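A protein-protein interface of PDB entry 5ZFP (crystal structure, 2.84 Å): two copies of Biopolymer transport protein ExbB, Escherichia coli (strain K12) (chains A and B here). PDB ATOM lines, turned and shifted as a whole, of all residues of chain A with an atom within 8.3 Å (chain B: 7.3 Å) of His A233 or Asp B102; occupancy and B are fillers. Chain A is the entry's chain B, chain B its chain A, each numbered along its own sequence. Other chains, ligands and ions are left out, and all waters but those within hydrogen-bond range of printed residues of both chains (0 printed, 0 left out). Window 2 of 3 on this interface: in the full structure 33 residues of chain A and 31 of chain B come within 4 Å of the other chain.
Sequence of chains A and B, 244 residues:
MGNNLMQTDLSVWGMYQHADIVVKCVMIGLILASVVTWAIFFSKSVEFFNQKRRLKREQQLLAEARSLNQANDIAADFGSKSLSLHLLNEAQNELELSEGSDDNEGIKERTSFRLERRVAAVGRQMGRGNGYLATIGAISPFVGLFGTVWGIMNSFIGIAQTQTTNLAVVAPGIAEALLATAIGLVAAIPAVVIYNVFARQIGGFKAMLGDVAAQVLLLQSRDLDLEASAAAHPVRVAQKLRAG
The side-chain carboxylate (OD1) of Asp B102 lies within hydrogen-bond range of a ring nitrogen (NE2) of His A233 (2.9 Å). The side-chain hydroxyl of Ser A229 is in hydrogen-bond range of the backbone NH of Asp B102, at 2.9 Å.
The side-chain hydroxyl (OG) of Ser B101 is in hydrogen-bond range of the backbone NH (N) of Asp B103, at 3.3 Å. The backbone NH of Glu B105 lies close to the side-chain carboxylate of Asp B103 (3.5 Å). NE2 of His A233 lies within hydrogen-bond range of O of Ser A229 (3.0 Å). The side-chain hydroxyl (OG) of Ser A229 lies within hydrogen-bond range of the backbone carbonyl oxygen (O) of Asp A225, 2.8 Å away.
Asp A225 touches Ser B101. Asp B103 touches Asp A225. Asp A225 touches Gly B106. O of Ser B98 touches CD2 of Leu A226, at 3.6 Å. Glu B99 touches Leu A226 (O to CD2, 3.5 Å). CD2 of Leu A226 touches C of Gly B100 (3.7 Å). Ser B101 touches Leu A226 (N to CD2, 3.6 Å). O of Gly B100 touches CB of Ser A229, 3.3 Å away. Ser A229 touches Ser B101 (OG to CA, 3.5 Å).
Ala A228 touches none of the printed residues of chain B. Printed residues of chain B within 4 Å of Ser A229: Gly B100, Ser B101 and Asp B102. His A233 touches just one residue of chain B: Asp B102. Printed residues of chain A within 4 Å of Glu B99: Leu A226. Of the printed residues of chain A, Gly B100 touches Leu A226 (3.7 Å) and Ser A229 (3.3 Å). Of chain A, only Asp A225, Leu A226 and Ser A229 come within 4 Å of Ser B101. Asp B102 touches just these residues of chain A: Ser A229 and His A233. Of the printed residues of chain A, Asp B103 touches Asp A225 (3.6 Å). Glu B105 touches none of the printed residues of chain A.
Hydrophobic or aromatic side chains of chain A that line the printed part of chain B: Leu A226 and His A233. Of the 10 printed residues of chain B, 7 touch a printed residue of chain A. Among the printed residues, 11 pairs touch across the chains. Among the printed residues, no Asp or Glu carboxylate lies within 4 Å of a Lys or Arg side-chain nitrogen of the other chain.
No position is printed for both chains. Of the 11 pairs that touch across the chains among the printed residues, none has its exchanged pair printed and touching as well.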
ATOM      1  N   ASP A 225       7.348  -4.301   8.398  1.00  0.00           N
ATOM      2  CA  ASP A 225       7.083  -3.361   9.489  1.00  0.00           C
ATOM      3  C   ASP A 225       5.988  -3.855  10.430  1.00  0.00           C
ATOM      4  O   ASP A 225       6.122  -3.706  11.648  1.00  0.00           O
ATOM      5  CB  ASP A 225       6.729  -1.962   8.928  1.00  0.00           C
ATOM      6  CG  ASP A 225       7.906  -1.145   8.434  1.00  0.00           C
ATOM      7  OD1 ASP A 225       9.009  -1.712   8.297  1.00  0.00           O
ATOM      8  OD2 ASP A 225       7.730   0.064   8.203  1.00  0.00           O
ATOM      9  N   LEU A 226       4.896  -4.420   9.865  1.00  0.00           N
ATOM     10  CA  LEU A 226       3.766  -4.932  10.639  1.00  0.00           C
ATOM     11  C   LEU A 226       4.149  -6.209  11.383  1.00  0.00           C
ATOM     12  O   LEU A 226       3.663  -6.423  12.489  1.00  0.00           O
ATOM     13  CB  LEU A 226       2.533  -5.152   9.753  1.00  0.00           C
ATOM     14  CG  LEU A 226       1.877  -3.901   9.138  1.00  0.00           C
ATOM     15  CD1 LEU A 226       0.999  -4.285   7.990  1.00  0.00           C
ATOM     16  CD2 LEU A 226       1.099  -3.070  10.171  1.00  0.00           C
ATOM     17  N   GLU A 227       5.045  -7.034  10.795  1.00  0.00           N
ATOM     18  CA  GLU A 227       5.589  -8.277  11.359  1.00  0.00           C
ATOM     19  C   GLU A 227       6.489  -7.945  12.558  1.00  0.00           C
ATOM     20  O   GLU A 227       6.381  -8.596  13.594  1.00  0.00           O
ATOM     21  CB  GLU A 227       6.391  -9.030  10.277  1.00  0.00           C
ATOM     22  CG  GLU A 227       6.907 -10.405  10.671  1.00  0.00           C
ATOM     23  CD  GLU A 227       7.921 -11.041   9.733  1.00  0.00           C
ATOM     24  OE1 GLU A 227       8.942 -10.389   9.403  1.00  0.00           O
ATOM     25  OE2 GLU A 227       7.729 -12.229   9.390  1.00  0.00           O
ATOM     26  N   ALA A 228       7.360  -6.927  12.414  1.00  0.00           N
ATOM     27  CA  ALA A 228       8.277  -6.468  13.449  1.00  0.00           C
ATOM     28  C   ALA A 228       7.528  -5.844  14.637  1.00  0.00           C
ATOM     29  O   ALA A 228       7.979  -5.962  15.776  1.00  0.00           O
ATOM     30  CB  ALA A 228       9.266  -5.478  12.856  1.00  0.00           C
ATOM     31  N   SER A 229       6.392  -5.191  14.366  1.00  0.00           N
ATOM     32  CA  SER A 229       5.541  -4.555  15.372  1.00  0.00           C
ATOM     33  C   SER A 229       4.792  -5.602  16.200  1.00  0.00           C
ATOM     34  O   SER A 229       4.591  -5.399  17.393  1.00  0.00           O
ATOM     35  CB  SER A 229       4.555  -3.605  14.706  1.00  0.00           C
ATOM     36  OG  SER A 229       5.240  -2.555  14.041  1.00  0.00           O
ATOM     37  N   ALA A 230       4.410  -6.730  15.567  1.00  0.00           N
ATOM     38  CA  ALA A 230       3.706  -7.852  16.192  1.00  0.00           C
ATOM     39  C   ALA A 230       4.622  -8.639  17.130  1.00  0.00           C
ATOM     40  O   ALA A 230       4.137  -9.230  18.098  1.00  0.00           O
ATOM     41  CB  ALA A 230       3.139  -8.776  15.124  1.00  0.00           C
ATOM     42  N   ALA A 231       5.932  -8.652  16.835  1.00  0.00           N
ATOM     43  CA  ALA A 231       6.952  -9.332  17.627  1.00  0.00           C
ATOM     44  C   ALA A 231       7.367  -8.488  18.858  1.00  0.00           C
ATOM     45  O   ALA A 231       7.666  -9.051  19.913  1.00  0.00           O
ATOM     46  CB  ALA A 231       8.160  -9.633  16.756  1.00  0.00           C
ATOM     47  N   ALA A 232       7.385  -7.147  18.710  1.00  0.00           N
ATOM     48  CA  ALA A 232       7.742  -6.185  19.751  1.00  0.00           C
ATOM     49  C   ALA A 232       6.697  -6.121  20.870  1.00  0.00           C
ATOM     50  O   ALA A 232       7.066  -5.926  22.030  1.00  0.00           O
ATOM     51  CB  ALA A 232       7.932  -4.811  19.140  1.00  0.00           C
ATOM     52  N   HIS A 233       5.400  -6.257  20.522  1.00  0.00           N
ATOM     53  CA  HIS A 233       4.305  -6.237  21.495  1.00  0.00           C
ATOM     54  C   HIS A 233       3.268  -7.357  21.230  1.00  0.00           C
ATOM     55  O   HIS A 233       2.210  -7.104  20.639  1.00  0.00           O
ATOM     56  CB  HIS A 233       3.657  -4.841  21.632  1.00  0.00           C
ATOM     57  CG  HIS A 233       3.293  -4.185  20.336  1.00  0.00           C
ATOM     58  ND1 HIS A 233       2.100  -4.471  19.688  1.00  0.00           N
ATOM     59  CD2 HIS A 233       3.962  -3.246  19.627  1.00  0.00           C
ATOM     60  CE1 HIS A 233       2.094  -3.721  18.599  1.00  0.00           C
ATOM     61  NE2 HIS A 233       3.195  -2.968  18.517  1.00  0.00           N
ATOM     62  N   PRO A 234       3.553  -8.613  21.664  1.00  0.00           N
ATOM     63  CA  PRO A 234       2.585  -9.699  21.435  1.00  0.00           C
ATOM     64  C   PRO A 234       1.495  -9.741  22.505  1.00  0.00           C
ATOM     65  O   PRO A 234       0.763  -8.770  22.691  1.00  0.00           O
ATOM     66  CB  PRO A 234       3.452 -10.967  21.441  1.00  0.00           C
ATOM     67  CG  PRO A 234       4.803 -10.552  21.993  1.00  0.00           C
ATOM     68  CD  PRO A 234       4.744  -9.107  22.385  1.00  0.00           C
ATOM     69  N   SER B  98      -1.222   0.373   6.919  1.00  0.00           N
ATOM     70  CA  SER B  98      -0.138   0.373   7.904  1.00  0.00           C
ATOM     71  C   SER B  98      -0.660   0.343   9.342  1.00  0.00           C
ATOM     72  O   SER B  98       0.144   0.443  10.271  1.00  0.00           O
ATOM     73  CB  SER B  98       0.757   1.595   7.722  1.00  0.00           C
ATOM     74  OG  SER B  98       1.292   1.694   6.415  1.00  0.00           O
ATOM     75  N   GLU B  99      -1.998   0.212   9.532  1.00  0.00           N
ATOM     76  CA  GLU B  99      -2.630   0.136  10.861  1.00  0.00           C
ATOM     77  C   GLU B  99      -2.040  -1.049  11.635  1.00  0.00           C
ATOM     78  O   GLU B  99      -2.092  -2.195  11.175  1.00  0.00           O
ATOM     79  CB  GLU B  99      -4.158   0.026  10.756  1.00  0.00           C
ATOM     80  CG  GLU B  99      -4.895   0.822  11.817  1.00  0.00           C
ATOM     81  CD  GLU B  99      -5.163   2.273  11.464  1.00  0.00           C
ATOM     82  OE1 GLU B  99      -4.430   3.159  11.964  1.00  0.00           O
ATOM     83  OE2 GLU B  99      -6.116   2.528  10.693  1.00  0.00           O
ATOM     84  N   GLY B 100      -1.389  -0.726  12.746  1.00  0.00           N
ATOM     85  CA  GLY B 100      -0.717  -1.695  13.601  1.00  0.00           C
ATOM     86  C   GLY B 100       0.800  -1.656  13.546  1.00  0.00           C
ATOM     87  O   GLY B 100       1.457  -2.515  14.140  1.00  0.00           O
ATOM     88  N   SER B 101       1.371  -0.662  12.840  1.00  0.00           N
ATOM     89  CA  SER B 101       2.812  -0.493  12.698  1.00  0.00           C
ATOM     90  C   SER B 101       3.352   0.552  13.669  1.00  0.00           C
ATOM     91  O   SER B 101       2.760   1.622  13.831  1.00  0.00           O
ATOM     92  CB  SER B 101       3.169  -0.126  11.261  1.00  0.00           C
ATOM     93  OG  SER B 101       4.557   0.097  11.090  1.00  0.00           O
ATOM     94  N   ASP B 102       4.492   0.233  14.291  1.00  0.00           N
ATOM     95  CA  ASP B 102       5.232   1.086  15.222  1.00  0.00           C
ATOM     96  C   ASP B 102       6.196   2.034  14.481  1.00  0.00           C
ATOM     97  O   ASP B 102       6.626   3.031  15.072  1.00  0.00           O
ATOM     98  CB  ASP B 102       6.036   0.223  16.212  1.00  0.00           C
ATOM     99  CG  ASP B 102       5.228  -0.744  17.061  1.00  0.00           C
ATOM    100  OD1 ASP B 102       4.017  -0.471  17.303  1.00  0.00           O
ATOM    101  OD2 ASP B 102       5.813  -1.748  17.528  1.00  0.00           O
ATOM    102  N   ASP B 103       6.554   1.717  13.207  1.00  0.00           N
ATOM    103  CA  ASP B 103       7.470   2.528  12.401  1.00  0.00           C
ATOM    104  C   ASP B 103       6.746   3.644  11.618  1.00  0.00           C
ATOM    105  O   ASP B 103       6.215   3.413  10.526  1.00  0.00           O
ATOM    106  CB  ASP B 103       8.341   1.643  11.489  1.00  0.00           C
ATOM    107  CG  ASP B 103       9.615   2.287  10.951  1.00  0.00           C
ATOM    108  OD1 ASP B 103       9.903   3.450  11.323  1.00  0.00           O
ATOM    109  OD2 ASP B 103      10.334   1.618  10.167  1.00  0.00           O
ATOM    110  N   ASN B 104       6.723   4.857  12.203  1.00  0.00           N
ATOM    111  CA  ASN B 104       6.100   6.044  11.622  1.00  0.00           C
ATOM    112  C   ASN B 104       6.889   6.565  10.433  1.00  0.00           C
ATOM    113  O   ASN B 104       6.297   7.126   9.509  1.00  0.00           O
ATOM    114  CB  ASN B 104       5.944   7.140  12.676  1.00  0.00           C
ATOM    115  CG  ASN B 104       4.674   7.078  13.505  1.00  0.00           C
ATOM    116  OD1 ASN B 104       3.928   6.097  13.504  1.00  0.00           O
ATOM    117  ND2 ASN B 104       4.391   8.140  14.233  1.00  0.00           N
ATOM    118  N   GLU B 105       8.226   6.371  10.449  1.00  0.00           N
ATOM    119  CA  GLU B 105       9.125   6.793   9.375  1.00  0.00           C
ATOM    120  C   GLU B 105       8.858   5.997   8.109  1.00  0.00           C
ATOM    121  O   GLU B 105       8.909   6.557   7.016  1.00  0.00           O
ATOM    122  CB  GLU B 105      10.595   6.699   9.812  1.00  0.00           C
ATOM    123  CG  GLU B 105      11.480   7.787   9.217  1.00  0.00           C
ATOM    124  CD  GLU B 105      11.148   9.243   9.522  1.00  0.00           C
ATOM    125  OE1 GLU B 105      11.365  10.093   8.626  1.00  0.00           O
ATOM    126  OE2 GLU B 105      10.673   9.538  10.646  1.00  0.00           O
ATOM    127  N   GLY B 106       8.518   4.721   8.276  1.00  0.00           N
ATOM    128  CA  GLY B 106       8.153   3.824   7.191  1.00  0.00           C
ATOM    129  C   GLY B 106       6.863   4.246   6.512  1.00  0.00           C
ATOM    130  O   GLY B 106       6.736   4.089   5.299  1.00  0.00           O
ATOM    131  N   ILE B 107       5.895   4.794   7.285  1.00  0.00           N
ATOM    132  CA  ILE B 107       4.610   5.276   6.760  1.00  0.00           C
ATOM    133  C   ILE B 107       4.863   6.519   5.891  1.00  0.00           C
ATOM    134  O   ILE B 107       4.383   6.580   4.754  1.00  0.00           O
ATOM    135  CB  ILE B 107       3.553   5.521   7.887  1.00  0.00           C
ATOM    136  CG1 ILE B 107       3.243   4.209   8.649  1.00  0.00           C
ATOM    137  CG2 ILE B 107       2.261   6.145   7.319  1.00  0.00           C
ATOM    138  CD1 ILE B 107       2.515   4.351   9.948  1.00  0.00           C
